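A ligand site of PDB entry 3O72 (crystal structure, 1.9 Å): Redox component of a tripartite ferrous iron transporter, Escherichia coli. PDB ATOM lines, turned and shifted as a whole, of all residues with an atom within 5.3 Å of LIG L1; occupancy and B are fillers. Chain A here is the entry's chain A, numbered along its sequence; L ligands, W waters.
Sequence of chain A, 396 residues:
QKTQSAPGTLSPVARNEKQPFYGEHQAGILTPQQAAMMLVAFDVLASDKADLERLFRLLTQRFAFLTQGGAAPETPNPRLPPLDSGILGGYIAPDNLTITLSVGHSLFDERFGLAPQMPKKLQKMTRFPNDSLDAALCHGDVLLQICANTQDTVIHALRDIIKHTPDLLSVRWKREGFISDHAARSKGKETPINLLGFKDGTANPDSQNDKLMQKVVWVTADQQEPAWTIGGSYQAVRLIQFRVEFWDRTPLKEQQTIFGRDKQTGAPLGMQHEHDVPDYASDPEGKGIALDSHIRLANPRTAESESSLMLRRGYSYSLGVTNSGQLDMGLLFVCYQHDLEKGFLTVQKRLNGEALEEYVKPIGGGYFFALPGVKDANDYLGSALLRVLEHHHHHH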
ATOM      1  N   ASN A 194      -8.307   6.213 -23.542  1.00  0.00           N
ATOM      2  CA  ASN A 194      -7.508   5.405 -22.611  1.00  0.00           C
ATOM      3  C   ASN A 194      -6.308   4.803 -23.313  1.00  0.00           C
ATOM      4  O   ASN A 194      -6.147   4.947 -24.519  1.00  0.00           O
ATOM      5  CB  ASN A 194      -8.363   4.324 -21.924  1.00  0.00           C
ATOM      6  CG  ASN A 194      -8.907   3.274 -22.909  1.00  0.00           C
ATOM      7  OD1 ASN A 194      -8.316   3.032 -23.969  1.00  0.00           O
ATOM      8  ND2 ASN A 194     -10.041   2.677 -22.555  1.00  0.00           N
ATOM      9  N   LEU A 196      -5.554   1.863 -24.126  1.00  0.00           N
ATOM     10  CA  LEU A 196      -5.881   0.835 -25.135  1.00  0.00           C
ATOM     11  C   LEU A 196      -6.307   1.498 -26.443  1.00  0.00           C
ATOM     12  O   LEU A 196      -6.619   0.828 -27.429  1.00  0.00           O
ATOM     13  CB  LEU A 196      -7.027  -0.073 -24.634  1.00  0.00           C
ATOM     14  CG  LEU A 196      -6.681  -0.893 -23.394  1.00  0.00           C
ATOM     15  CD1 LEU A 196      -7.850  -1.767 -22.962  1.00  0.00           C
ATOM     16  CD2 LEU A 196      -5.423  -1.744 -23.633  1.00  0.00           C
ATOM     17  N   PHE A 198      -9.059   3.420 -26.875  1.00  0.00           N
ATOM     18  CA  PHE A 198     -10.490   3.639 -27.026  1.00  0.00           C
ATOM     19  C   PHE A 198     -10.953   4.851 -26.225  1.00  0.00           C
ATOM     20  O   PHE A 198     -10.434   5.113 -25.145  1.00  0.00           O
ATOM     21  CB  PHE A 198     -11.293   2.397 -26.599  1.00  0.00           C
ATOM     22  CG  PHE A 198     -11.361   1.335 -27.653  1.00  0.00           C
ATOM     23  CD1 PHE A 198     -10.254   0.554 -27.938  1.00  0.00           C
ATOM     24  CD2 PHE A 198     -12.548   1.120 -28.352  1.00  0.00           C
ATOM     25  CE1 PHE A 198     -10.306  -0.420 -28.937  1.00  0.00           C
ATOM     26  CE2 PHE A 198     -12.609   0.146 -29.347  1.00  0.00           C
ATOM     27  CZ  PHE A 198     -11.491  -0.625 -29.633  1.00  0.00           C
ATOM     28  N   LYS A 199     -11.943   5.555 -26.759  1.00  0.00           N
ATOM     29  CA  LYS A 199     -12.581   6.648 -26.025  1.00  0.00           C
ATOM     30  C   LYS A 199     -13.257   6.037 -24.815  1.00  0.00           C
ATOM     31  O   LYS A 199     -13.868   4.962 -24.909  1.00  0.00           O
ATOM     32  CB  LYS A 199     -13.625   7.363 -26.879  1.00  0.00           C
ATOM     33  CG  LYS A 199     -13.090   8.044 -28.139  1.00  0.00           C
ATOM     34  CD  LYS A 199     -14.258   8.525 -29.017  1.00  0.00           C
ATOM     35  CE  LYS A 199     -13.875   9.685 -29.923  1.00  0.00           C
ATOM     36  NZ  LYS A 199     -12.737   9.366 -30.822  1.00  0.00           N
ATOM     37  N   ASP A 200     -13.157   6.726 -23.683  1.00  0.00           N
ATOM     38  CA  ASP A 200     -13.553   6.181 -22.394  1.00  0.00           C
ATOM     39  C   ASP A 200     -14.285   7.263 -21.597  1.00  0.00           C
ATOM     40  O   ASP A 200     -13.661   8.214 -21.126  1.00  0.00           O
ATOM     41  CB  ASP A 200     -12.304   5.721 -21.648  1.00  0.00           C
ATOM     42  CG  ASP A 200     -12.592   4.749 -20.525  1.00  0.00           C
ATOM     43  OD1 ASP A 200     -13.693   4.843 -19.912  1.00  0.00           O
ATOM     44  OD2 ASP A 200     -11.733   3.886 -20.253  1.00  0.00           O
ATOM     45  N   GLY A 201     -15.588   7.095 -21.442  1.00  0.00           N
ATOM     46  CA  GLY A 201     -16.422   8.085 -20.785  1.00  0.00           C
ATOM     47  C   GLY A 201     -17.702   8.377 -21.551  1.00  0.00           C
ATOM     48  O   GLY A 201     -18.646   8.947 -21.015  1.00  0.00           O
ATOM     49  N   THR A 202     -17.745   7.964 -22.813  1.00  0.00           N
ATOM     50  CA  THR A 202     -18.863   8.266 -23.722  1.00  0.00           C
ATOM     51  C   THR A 202     -20.268   8.172 -23.108  1.00  0.00           C
ATOM     52  O   THR A 202     -21.051   9.137 -23.141  1.00  0.00           O
ATOM     53  CB  THR A 202     -18.821   7.385 -24.977  1.00  0.00           C
ATOM     54  OG1 THR A 202     -17.514   7.457 -25.563  1.00  0.00           O
ATOM     55  CG2 THR A 202     -19.871   7.839 -25.992  1.00  0.00           C
ATOM     56  N   ALA A 203     -20.609   7.013 -22.549  1.00  0.00           N
ATOM     57  CA  ALA A 203     -21.958   6.767 -22.071  1.00  0.00           C
ATOM     58  C   ALA A 203     -22.220   7.172 -20.618  1.00  0.00           C
ATOM     59  O   ALA A 203     -23.231   6.787 -20.037  1.00  0.00           O
ATOM     60  CB  ALA A 203     -22.336   5.308 -22.295  1.00  0.00           C
ATOM     61  N   ASN A 204     -21.305   7.944 -20.019  1.00  0.00           N
ATOM     62  CA  ASN A 204     -21.512   8.462 -18.670  1.00  0.00           C
ATOM     63  C   ASN A 204     -22.807   9.272 -18.609  1.00  0.00           C
ATOM     64  O   ASN A 204     -23.100   9.992 -19.546  1.00  0.00           O
ATOM     65  CB  ASN A 204     -20.355   9.392 -18.314  1.00  0.00           C
ATOM     66  CG  ASN A 204     -19.452   8.858 -17.218  1.00  0.00           C
ATOM     67  OD1 ASN A 204     -19.848   8.007 -16.439  1.00  0.00           O
ATOM     68  ND2 ASN A 204     -18.246   9.401 -17.139  1.00  0.00           N
ATOM     69  N   ARG A 238     -10.566   0.985  -8.521  1.00  0.00           N
ATOM     70  CA  ARG A 238      -9.898  -0.222  -9.003  1.00  0.00           C
ATOM     71  C   ARG A 238      -8.628   0.163  -9.752  1.00  0.00           C
ATOM     72  O   ARG A 238      -8.679   0.940 -10.710  1.00  0.00           O
ATOM     73  CB  ARG A 238     -10.817  -1.055  -9.920  1.00  0.00           C
ATOM     74  CG  ARG A 238     -12.128  -1.501  -9.266  1.00  0.00           C
ATOM     75  CD  ARG A 238     -11.963  -2.805  -8.498  1.00  0.00           C
ATOM     76  NE  ARG A 238     -11.967  -3.944  -9.422  1.00  0.00           N
ATOM     77  CZ  ARG A 238     -11.692  -5.195  -9.085  1.00  0.00           C
ATOM     78  NH1 ARG A 238     -11.368  -5.509  -7.837  1.00  0.00           N
ATOM     79  NH2 ARG A 238     -11.733  -6.151 -10.003  1.00  0.00           N
ATOM     80  N   ILE A 240      -6.102  -1.081 -12.277  1.00  0.00           N
ATOM     81  CA  ILE A 240      -6.182  -2.103 -13.314  1.00  0.00           C
ATOM     82  C   ILE A 240      -5.040  -1.974 -14.323  1.00  0.00           C
ATOM     83  O   ILE A 240      -4.919  -0.977 -15.037  1.00  0.00           O
ATOM     84  CB  ILE A 240      -7.555  -2.054 -14.051  1.00  0.00           C
ATOM     85  CG1 ILE A 240      -8.698  -2.206 -13.038  1.00  0.00           C
ATOM     86  CG2 ILE A 240      -7.667  -3.186 -15.091  1.00  0.00           C
ATOM     87  CD1 ILE A 240     -10.059  -1.920 -13.646  1.00  0.00           C
ATOM     88  N   PHE A 242      -2.847  -3.118 -17.675  1.00  0.00           N
ATOM     89  CA  PHE A 242      -3.117  -3.576 -19.050  1.00  0.00           C
ATOM     90  C   PHE A 242      -1.992  -4.452 -19.583  1.00  0.00           C
ATOM     91  O   PHE A 242      -0.821  -4.226 -19.274  1.00  0.00           O
ATOM     92  CB  PHE A 242      -3.245  -2.399 -20.039  1.00  0.00           C
ATOM     93  CG  PHE A 242      -4.385  -1.479 -19.785  1.00  0.00           C
ATOM     94  CD1 PHE A 242      -5.407  -1.831 -18.924  1.00  0.00           C
ATOM     95  CD2 PHE A 242      -4.419  -0.234 -20.419  1.00  0.00           C
ATOM     96  CE1 PHE A 242      -6.467  -0.959 -18.703  1.00  0.00           C
ATOM     97  CE2 PHE A 242      -5.476   0.635 -20.222  1.00  0.00           C
ATOM     98  CZ  PHE A 242      -6.497   0.291 -19.359  1.00  0.00           C
ATOM     99  N   PHE A 259     -14.801  -4.530 -26.999  1.00  0.00           N
ATOM    100  CA  PHE A 259     -15.488  -3.368 -26.414  1.00  0.00           C
ATOM    101  C   PHE A 259     -16.944  -3.184 -26.855  1.00  0.00           C
ATOM    102  O   PHE A 259     -17.789  -2.832 -26.037  1.00  0.00           O
ATOM    103  CB  PHE A 259     -14.668  -2.088 -26.602  1.00  0.00           C
ATOM    104  CG  PHE A 259     -13.580  -1.942 -25.581  1.00  0.00           C
ATOM    105  CD1 PHE A 259     -13.895  -1.789 -24.247  1.00  0.00           C
ATOM    106  CD2 PHE A 259     -12.237  -2.017 -25.951  1.00  0.00           C
ATOM    107  CE1 PHE A 259     -12.903  -1.687 -23.273  1.00  0.00           C
ATOM    108  CE2 PHE A 259     -11.236  -1.930 -25.007  1.00  0.00           C
ATOM    109  CZ  PHE A 259     -11.572  -1.759 -23.649  1.00  0.00           C
ATOM    110  N   ARG A 261     -17.488  -1.192 -29.528  1.00  0.00           N
ATOM    111  CA  ARG A 261     -17.425   0.127 -30.149  1.00  0.00           C
ATOM    112  C   ARG A 261     -16.358   0.228 -31.240  1.00  0.00           C
ATOM    113  O   ARG A 261     -15.351  -0.498 -31.230  1.00  0.00           O
ATOM    114  CB  ARG A 261     -17.219   1.230 -29.107  1.00  0.00           C
ATOM    115  CG  ARG A 261     -18.463   1.484 -28.248  1.00  0.00           C
ATOM    116  CD  ARG A 261     -18.351   2.738 -27.434  1.00  0.00           C
ATOM    117  NE  ARG A 261     -19.539   2.995 -26.626  1.00  0.00           N
ATOM    118  CZ  ARG A 261     -20.514   3.829 -26.946  1.00  0.00           C
ATOM    119  NH1 ARG A 261     -20.471   4.513 -28.089  1.00  0.00           N
ATOM    120  NH2 ARG A 261     -21.547   3.995 -26.134  1.00  0.00           N
ATOM    121  N   TYR A 280     -30.001  -3.252 -28.453  1.00  0.00           N
ATOM    122  CA  TYR A 280     -29.680  -4.658 -28.193  1.00  0.00           C
ATOM    123  C   TYR A 280     -30.854  -5.577 -28.539  1.00  0.00           C
ATOM    124  O   TYR A 280     -30.664  -6.718 -28.912  1.00  0.00           O
ATOM    125  CB  TYR A 280     -29.204  -4.872 -26.755  1.00  0.00           C
ATOM    126  CG  TYR A 280     -27.904  -4.158 -26.431  1.00  0.00           C
ATOM    127  CD1 TYR A 280     -27.722  -3.505 -25.218  1.00  0.00           C
ATOM    128  CD2 TYR A 280     -26.870  -4.101 -27.371  1.00  0.00           C
ATOM    129  CE1 TYR A 280     -26.523  -2.850 -24.922  1.00  0.00           C
ATOM    130  CE2 TYR A 280     -25.674  -3.443 -27.084  1.00  0.00           C
ATOM    131  CZ  TYR A 280     -25.506  -2.818 -25.874  1.00  0.00           C
ATOM    132  OH  TYR A 280     -24.339  -2.158 -25.577  1.00  0.00           O
ATOM    133  N   HIS A 294     -17.659  -5.580 -23.600  1.00  0.00           N
ATOM    134  CA  HIS A 294     -17.594  -4.780 -22.386  1.00  0.00           C
ATOM    135  C   HIS A 294     -18.849  -3.938 -22.196  1.00  0.00           C
ATOM    136  O   HIS A 294     -19.453  -3.951 -21.115  1.00  0.00           O
ATOM    137  CB  HIS A 294     -16.337  -3.915 -22.408  1.00  0.00           C
ATOM    138  CG  HIS A 294     -16.142  -3.115 -21.162  1.00  0.00           C
ATOM    139  ND1 HIS A 294     -15.775  -3.695 -19.972  1.00  0.00           N
ATOM    140  CD2 HIS A 294     -16.302  -1.788 -20.916  1.00  0.00           C
ATOM    141  CE1 HIS A 294     -15.689  -2.760 -19.043  1.00  0.00           C
ATOM    142  NE2 HIS A 294     -16.007  -1.593 -19.592  1.00  0.00           N
ATOM    143  N   ILE A 295     -19.292  -3.222 -23.215  1.00  0.00           N
ATOM    144  CA  ILE A 295     -20.391  -2.278 -23.000  1.00  0.00           C
ATOM    145  C   ILE A 295     -21.753  -2.940 -22.843  1.00  0.00           C
ATOM    146  O   ILE A 295     -22.580  -2.490 -22.054  1.00  0.00           O
ATOM    147  CB  ILE A 295     -20.425  -1.178 -24.037  1.00  0.00           C
ATOM    148  CG1 ILE A 295     -20.871  -1.711 -25.408  1.00  0.00           C
ATOM    149  CG2 ILE A 295     -19.065  -0.443 -24.070  1.00  0.00           C
ATOM    150  CD1 ILE A 295     -21.153  -0.605 -26.422  1.00  0.00           C
ATOM    151  N   ALA A 298     -21.761  -4.185 -19.336  1.00  0.00           N
ATOM    152  CA  ALA A 298     -21.746  -3.089 -18.374  1.00  0.00           C
ATOM    153  C   ALA A 298     -23.116  -2.459 -18.334  1.00  0.00           C
ATOM    154  O   ALA A 298     -23.615  -2.118 -17.273  1.00  0.00           O
ATOM    155  CB  ALA A 298     -20.707  -2.054 -18.729  1.00  0.00           C
ATOM    156  N   ASN A 299     -23.742  -2.335 -19.494  1.00  0.00           N
ATOM    157  CA  ASN A 299     -25.046  -1.699 -19.564  1.00  0.00           C
ATOM    158  C   ASN A 299     -25.931  -2.414 -20.553  1.00  0.00           C
ATOM    159  O   ASN A 299     -25.878  -2.145 -21.758  1.00  0.00           O
ATOM    160  CB  ASN A 299     -24.895  -0.216 -19.952  1.00  0.00           C
ATOM    161  CG  ASN A 299     -26.216   0.508 -19.943  1.00  0.00           C
ATOM    162  OD1 ASN A 299     -27.234  -0.074 -19.568  1.00  0.00           O
ATOM    163  ND2 ASN A 299     -26.209   1.774 -20.329  1.00  0.00           N
ATOM    164  N   ARG A 301     -28.938  -2.011 -20.983  1.00  0.00           N
ATOM    165  CA  ARG A 301     -29.941  -1.047 -21.460  1.00  0.00           C
ATOM    166  C   ARG A 301     -31.393  -1.577 -21.428  1.00  0.00           C
ATOM    167  O   ARG A 301     -32.163  -1.431 -22.375  1.00  0.00           O
ATOM    168  CB  ARG A 301     -29.574  -0.511 -22.853  1.00  0.00           C
ATOM    169  CG  ARG A 301     -28.255   0.248 -22.831  1.00  0.00           C
ATOM    170  CD  ARG A 301     -27.793   0.690 -24.210  1.00  0.00           C
ATOM    171  NE  ARG A 301     -26.474   1.319 -24.131  1.00  0.00           N
ATOM    172  CZ  ARG A 301     -26.289   2.605 -23.842  1.00  0.00           C
ATOM    173  NH1 ARG A 301     -27.333   3.391 -23.620  1.00  0.00           N
ATOM    174  NH2 ARG A 301     -25.065   3.111 -23.792  1.00  0.00           N
ATOM    175  N   MET A 310     -23.922   4.692 -12.992  1.00  0.00           N
ATOM    176  CA  MET A 310     -22.887   5.219 -12.105  1.00  0.00           C
ATOM    177  C   MET A 310     -22.205   6.353 -12.835  1.00  0.00           C
ATOM    178  O   MET A 310     -22.362   6.498 -14.030  1.00  0.00           O
ATOM    179  CB  MET A 310     -21.834   4.134 -11.839  1.00  0.00           C
ATOM    180  CG  MET A 310     -21.217   3.598 -13.115  1.00  0.00           C
ATOM    181  SD  MET A 310     -19.748   2.315 -12.815  1.00  0.00           S
ATOM    182  CE  MET A 310     -20.611   1.320 -11.422  1.00  0.00           C
ATOM    183  N   ARG A 312     -18.549   7.391 -13.834  1.00  0.00           N
ATOM    184  CA  ARG A 312     -17.140   7.019 -13.881  1.00  0.00           C
ATOM    185  C   ARG A 312     -16.262   8.252 -14.049  1.00  0.00           C
ATOM    186  O   ARG A 312     -16.601   9.188 -14.778  1.00  0.00           O
ATOM    187  CB  ARG A 312     -16.863   6.036 -15.029  1.00  0.00           C
ATOM    188  CG  ARG A 312     -17.469   4.649 -14.818  1.00  0.00           C
ATOM    189  CD  ARG A 312     -17.436   3.851 -16.142  1.00  0.00           C
ATOM    190  NE  ARG A 312     -18.358   4.396 -17.150  1.00  0.00           N
ATOM    191  CZ  ARG A 312     -18.050   4.657 -18.414  1.00  0.00           C
ATOM    192  NH1 ARG A 312     -16.809   4.441 -18.860  1.00  0.00           N
ATOM    193  NH2 ARG A 312     -18.969   5.128 -19.225  1.00  0.00           N
ATOM    194  N   LEU A 331      -5.327   1.674 -15.934  1.00  0.00           N
ATOM    195  CA  LEU A 331      -6.457   2.491 -15.574  1.00  0.00           C
ATOM    196  C   LEU A 331      -6.549   2.622 -14.070  1.00  0.00           C
ATOM    197  O   LEU A 331      -6.548   1.621 -13.344  1.00  0.00           O
ATOM    198  CB  LEU A 331      -7.735   1.822 -16.079  1.00  0.00           C
ATOM    199  CG  LEU A 331      -9.009   2.637 -15.935  1.00  0.00           C
ATOM    200  CD1 LEU A 331      -8.906   3.929 -16.757  1.00  0.00           C
ATOM    201  CD2 LEU A 331     -10.206   1.804 -16.389  1.00  0.00           C
ATOM    202  N   PHE A 333      -9.402   3.258 -12.238  1.00  0.00           N
ATOM    203  CA  PHE A 333     -10.851   3.319 -12.379  1.00  0.00           C
ATOM    204  C   PHE A 333     -11.426   3.873 -11.079  1.00  0.00           C
ATOM    205  O   PHE A 333     -11.093   3.391 -10.000  1.00  0.00           O
ATOM    206  CB  PHE A 333     -11.391   1.908 -12.674  1.00  0.00           C
ATOM    207  CG  PHE A 333     -12.881   1.821 -12.661  1.00  0.00           C
ATOM    208  CD1 PHE A 333     -13.608   1.886 -13.850  1.00  0.00           C
ATOM    209  CD2 PHE A 333     -13.575   1.659 -11.476  1.00  0.00           C
ATOM    210  CE1 PHE A 333     -14.977   1.794 -13.858  1.00  0.00           C
ATOM    211  CE2 PHE A 333     -14.964   1.581 -11.484  1.00  0.00           C
ATOM    212  CZ  PHE A 333     -15.660   1.641 -12.673  1.00  0.00           C
ATOM    213  N   PHE A 344     -21.558  -0.325  -8.628  1.00  0.00           N
ATOM    214  CA  PHE A 344     -20.363  -1.123  -8.905  1.00  0.00           C
ATOM    215  C   PHE A 344     -20.503  -2.627  -8.683  1.00  0.00           C
ATOM    216  O   PHE A 344     -20.123  -3.412  -9.537  1.00  0.00           O
ATOM    217  CB  PHE A 344     -19.153  -0.633  -8.113  1.00  0.00           C
ATOM    218  CG  PHE A 344     -17.892  -1.405  -8.416  1.00  0.00           C
ATOM    219  CD1 PHE A 344     -17.146  -1.099  -9.550  1.00  0.00           C
ATOM    220  CD2 PHE A 344     -17.466  -2.440  -7.606  1.00  0.00           C
ATOM    221  CE1 PHE A 344     -15.990  -1.807  -9.862  1.00  0.00           C
ATOM    222  CE2 PHE A 344     -16.304  -3.154  -7.900  1.00  0.00           C
ATOM    223  CZ  PHE A 344     -15.574  -2.841  -9.049  1.00  0.00           C
ATOM    224  N   VAL A 347     -22.675  -4.117 -11.472  1.00  0.00           N
ATOM    225  CA  VAL A 347     -22.078  -3.998 -12.793  1.00  0.00           C
ATOM    226  C   VAL A 347     -20.898  -4.970 -12.956  1.00  0.00           C
ATOM    227  O   VAL A 347     -20.792  -5.666 -13.963  1.00  0.00           O
ATOM    228  CB  VAL A 347     -21.631  -2.557 -13.099  1.00  0.00           C
ATOM    229  CG1 VAL A 347     -20.933  -2.485 -14.426  1.00  0.00           C
ATOM    230  CG2 VAL A 347     -22.853  -1.596 -13.102  1.00  0.00           C
ATOM    231  N   GLN A 348     -20.023  -5.024 -11.949  1.00  0.00           N
ATOM    232  CA  GLN A 348     -18.871  -5.911 -12.063  1.00  0.00           C
ATOM    233  C   GLN A 348     -19.327  -7.383 -12.064  1.00  0.00           C
ATOM    234  O   GLN A 348     -18.728  -8.239 -12.718  1.00  0.00           O
ATOM    235  CB  GLN A 348     -17.832  -5.628 -10.969  1.00  0.00           C
ATOM    236  CG  GLN A 348     -16.586  -6.560 -11.053  1.00  0.00           C
ATOM    237  CD  GLN A 348     -15.832  -6.457 -12.378  1.00  0.00           C
ATOM    238  OE1 GLN A 348     -15.464  -5.350 -12.798  1.00  0.00           O
ATOM    239  NE2 GLN A 348     -15.579  -7.606 -13.041  1.00  0.00           N
ATOM    240  N   LEU A 351     -19.995  -8.019 -15.474  1.00  0.00           N
ATOM    241  CA  LEU A 351     -18.753  -8.055 -16.239  1.00  0.00           C
ATOM    242  C   LEU A 351     -17.888  -9.310 -16.041  1.00  0.00           C
ATOM    243  O   LEU A 351     -17.059  -9.610 -16.882  1.00  0.00           O
ATOM    244  CB  LEU A 351     -17.900  -6.800 -15.960  1.00  0.00           C
ATOM    245  CG  LEU A 351     -18.449  -5.479 -16.500  1.00  0.00           C
ATOM    246  CD1 LEU A 351     -17.675  -4.271 -15.909  1.00  0.00           C
ATOM    247  CD2 LEU A 351     -18.383  -5.454 -18.022  1.00  0.00           C
ATOM    248  N   LEU A 356     -12.830  -8.956 -22.349  1.00  0.00           N
ATOM    249  CA  LEU A 356     -11.678  -8.133 -21.983  1.00  0.00           C
ATOM    250  C   LEU A 356     -10.723  -8.762 -20.958  1.00  0.00           C
ATOM    251  O   LEU A 356      -9.557  -8.384 -20.863  1.00  0.00           O
ATOM    252  CB  LEU A 356     -12.174  -6.794 -21.439  1.00  0.00           C
ATOM    253  CG  LEU A 356     -11.113  -5.744 -21.077  1.00  0.00           C
ATOM    254  CD1 LEU A 356     -10.284  -5.358 -22.292  1.00  0.00           C
ATOM    255  CD2 LEU A 356     -11.795  -4.510 -20.492  1.00  0.00           C
ATOM    256  N   VAL A 360      -6.566  -7.610 -19.002  1.00  0.00           N
ATOM    257  CA  VAL A 360      -6.469  -6.689 -17.871  1.00  0.00           C
ATOM    258  C   VAL A 360      -6.247  -7.425 -16.549  1.00  0.00           C
ATOM    259  O   VAL A 360      -6.586  -8.610 -16.408  1.00  0.00           O
ATOM    260  CB  VAL A 360      -7.730  -5.781 -17.767  1.00  0.00           C
ATOM    261  CG1 VAL A 360      -7.912  -4.952 -19.028  1.00  0.00           C
ATOM    262  CG2 VAL A 360      -8.986  -6.645 -17.513  1.00  0.00           C
HETATM  263  C1  LIG L   1     -17.850   1.828 -20.936  1.00  0.00           C
HETATM  264  C2  LIG L   1     -13.066   0.975 -21.017  1.00  0.00           C
HETATM  265  C3  LIG L   1     -13.452  -1.156 -16.648  1.00  0.00           C
HETATM  266  C4  LIG L   1     -18.095   0.158 -16.344  1.00  0.00           C
HETATM  267  C5  LIG L   1     -16.537   1.695 -21.348  1.00  0.00           C
HETATM  268  C6  LIG L   1     -16.049   2.043 -22.667  1.00  0.00           C
HETATM  269  C7  LIG L   1     -14.735   1.805 -22.681  1.00  0.00           C
HETATM  270  C8  LIG L   1     -14.351   1.318 -21.378  1.00  0.00           C
HETATM  271  C9  LIG L   1     -13.782   2.027 -23.871  1.00  0.00           C
HETATM  272  C10 LIG L   1     -16.890   2.569 -23.853  1.00  0.00           C
HETATM  273  C11 LIG L   1     -17.027   4.089 -23.874  1.00  0.00           C
HETATM  274  C12 LIG L   1     -17.835   4.581 -22.701  1.00  0.00           C
HETATM  275  O1  LIG L   1     -17.227   5.084 -21.718  1.00  0.00           O
HETATM  276  O2  LIG L   1     -19.099   4.478 -22.739  1.00  0.00           O
HETATM  277  C13 LIG L   1     -12.773   0.255 -19.881  1.00  0.00           C
HETATM  278  C14 LIG L   1     -11.532  -0.416 -19.601  1.00  0.00           C
HETATM  279  C15 LIG L   1     -11.648  -1.005 -18.412  1.00  0.00           C
HETATM  280  C16 LIG L   1     -12.966  -0.727 -17.874  1.00  0.00           C
HETATM  281  C17 LIG L   1     -10.288  -0.451 -20.532  1.00  0.00           C
HETATM  282  C18 LIG L   1     -10.557  -1.842 -17.724  1.00  0.00           C
HETATM  283  C19 LIG L   1     -10.917  -2.931 -17.058  1.00  0.00           C
HETATM  284  C20 LIG L   1     -14.722  -0.956 -16.164  1.00  0.00           C
HETATM  285  C21 LIG L   1     -15.238  -1.396 -14.876  1.00  0.00           C
HETATM  286  C22 LIG L   1     -16.524  -1.017 -14.815  1.00  0.00           C
HETATM  287  C23 LIG L   1     -16.864  -0.375 -16.060  1.00  0.00           C
HETATM  288  C24 LIG L   1     -14.450  -2.125 -13.759  1.00  0.00           C
HETATM  289  C25 LIG L   1     -17.569  -1.224 -13.699  1.00  0.00           C
HETATM  290  C26 LIG L   1     -17.472  -2.137 -12.735  1.00  0.00           C
HETATM  291  C27 LIG L   1     -18.462   0.738 -17.534  1.00  0.00           C
HETATM  292  C28 LIG L   1     -19.783   1.244 -17.851  1.00  0.00           C
HETATM  293  C29 LIG L   1     -19.699   1.745 -19.279  1.00  0.00           C
HETATM  294  C30 LIG L   1     -18.343   1.524 -19.701  1.00  0.00           C
HETATM  295  C31 LIG L   1     -21.023   1.271 -16.935  1.00  0.00           C
HETATM  296  C32 LIG L   1     -20.849   2.392 -20.086  1.00  0.00           C
HETATM  297  C33 LIG L   1     -21.510   1.283 -20.883  1.00  0.00           C
HETATM  298  C34 LIG L   1     -22.735   1.845 -21.559  1.00  0.00           C
HETATM  299  O3  LIG L   1     -22.876   1.684 -22.792  1.00  0.00           O
HETATM  300  O4  LIG L   1     -23.552   2.470 -20.838  1.00  0.00           O
HETATM  301  N1  LIG L   1     -15.477   1.248 -20.566  1.00  0.00           N
HETATM  302  N2  LIG L   1     -13.630   0.047 -18.808  1.00  0.00           N
HETATM  303  N3  LIG L   1     -15.740  -0.337 -16.870  1.00  0.00           N
HETATM  304  N4  LIG L   1     -17.648   0.914 -18.657  1.00  0.00           N
HETATM  305 FE1  LIG L   1     -15.651   0.324 -18.747  1.00  0.00          FE
HETATM  306  O1  LG2 L   2     -13.764   2.997 -17.654  1.00  0.00           O
HETATM  307  O2  LG2 L   2     -15.010   2.402 -17.947  1.00  0.00           O
HETATM  308  O   HOH W   1     -24.321   0.519 -16.299  1.00  0.00           O
HETATM  309  O   HOH W   2     -14.360  -4.943 -15.775  1.00  0.00           O
HETATM  310  O   HOH W   3     -24.430  -0.658 -23.693  1.00  0.00           O
HETATM  311  O   HOH W   4     -20.480   2.509 -23.854  1.00  0.00           O
HETATM  312  O   HOH W   5     -11.608  -5.011 -14.694  1.00  0.00           O
HETATM  313  O   HOH W   6     -24.019   4.030 -18.537  1.00  0.00           O
HETATM  314  O   HOH W   7     -12.834  -4.473 -12.152  1.00  0.00           O
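N of Leu 331 sits at hydrogen-bond distance from O of Ile 240 (2.8 Å).
OD1 of Asn 194 sits at hydrogen-bond distance from N of Phe 198, 3.0 Å away.
The backbone NH of Phe 333 sits at hydrogen-bond distance from the backbone carbonyl oxygen of Arg 238.
OD1 of Asn 299 is in hydrogen-bond range of N of Arg 301 (2.9 Å).
The side-chain carboxylate of Asp 200 is in hydrogen-bond range of the side-chain amide nitrogen of Asn 194 (3.1 Å).
The side-chain amide nitrogen (ND2) of Asn 204 lies within hydrogen-bond range of the backbone carbonyl oxygen (O) of Arg 312 (2.9 Å).
The backbone carbonyl oxygen (O) of Phe 259 lies within hydrogen-bond range of the backbone NH (N) of Ile 295 (3.2 Å).
The guanidinium group of Arg 312 is in salt-bridge range of the side-chain carboxylate of Asp 200.
Residues that only touch LIG L1: Lys 199 (3.1 Å), Phe 344 (3.2 Å), Asp 200 (3.3 Å), Phe 333 (3.3 Å), Phe 259 (3.5 Å), Gln 348 (3.5 Å), Ala 298 (3.5 Å), Leu 351 (3.6 Å), Ile 240 (3.7 Å), Val 347 (3.7 Å), Leu 196 (3.7 Å), Phe 198 (3.7 Å), Ile 295 (3.7 Å), Asn 194 (3.7 Å), Leu 331 (3.7 Å), Arg 261 (3.9 Å) and Leu 356 (3.9 Å).
Within 4 Å of LIG L1: Asn 194, Leu 196, Phe 198, Lys 199, Asp 200, Gly 201, Thr 202, Ala 203, Ile 240, Phe 259, Arg 261, His 294, Ile 295, Ala 298, Asn 299, Arg 301, Arg 312, Leu 331, Phe 333, Phe 344, Val 347, Gln 348, Leu 351 and Leu 356.
Along chain A the residues within 4 Å of LIG L1 span positions 194 to 356.
The nearest printed residue that does not touch LIG L1 is Phe 242 (4.04 Å).
Water W4 bridges an oxygen (O2) of LIG L1 and the guanidinium group of Arg 261.
Water W6 lies within hydrogen-bond range of O4 of LIG L1 (2.8 Å) and O of Ala 203 (3.2 Å).
Water W3 lies within hydrogen-bond range of the side-chain hydroxyl (OH) of Tyr 280 (2.4 Å), the backbone carbonyl oxygen (O) of Asn 299 (2.8 Å), the guanidinium group (NE) of Arg 301 (2.9 Å), an oxygen (O3) of LIG L1 (3.0 Å) and the backbone carbonyl oxygen (O) of Ile 295 (3.1 Å).
Water W7 lies within hydrogen-bond range of the side-chain amide oxygen (OE1) of Gln 348 (2.8 Å) and the guanidinium group (NE) of Arg 238 (2.9 Å).
N of Gly 201 is in hydrogen-bond range of O1 of LIG L1 (2.6 Å).
An oxygen (O4) of LIG L1 sits at hydrogen-bond distance from the side-chain amide nitrogen (ND2) of Asn 299, at 2.8 Å.
A ring nitrogen (NE2) of His 294 is bound to an iron atom (FE1) of LIG L1 (2.1 Å).
The guanidinium group of Arg 312 sits close to an oxygen (O2) of LG2 L2, 2.9 Å away.
The guanidinium group of Arg 312 lies within salt-bridge range of an oxygen (O1) of LIG L1 (3.0 Å).
The backbone NH of Thr 202 sits at hydrogen-bond distance from an oxygen (O1) of LIG L1, 3.1 Å away.
The backbone NH (N) of Ala 203 is in hydrogen-bond range of an oxygen (O2) of LIG L1, at 3.0 Å.
The guanidinium group of Arg 301 is in salt-bridge range of an oxygen (O3) of LIG L1, 2.8 Å away.
An oxygen (O2) of LG2 L2 binds an iron atom (FE1) of LIG L1 (2.3 Å).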
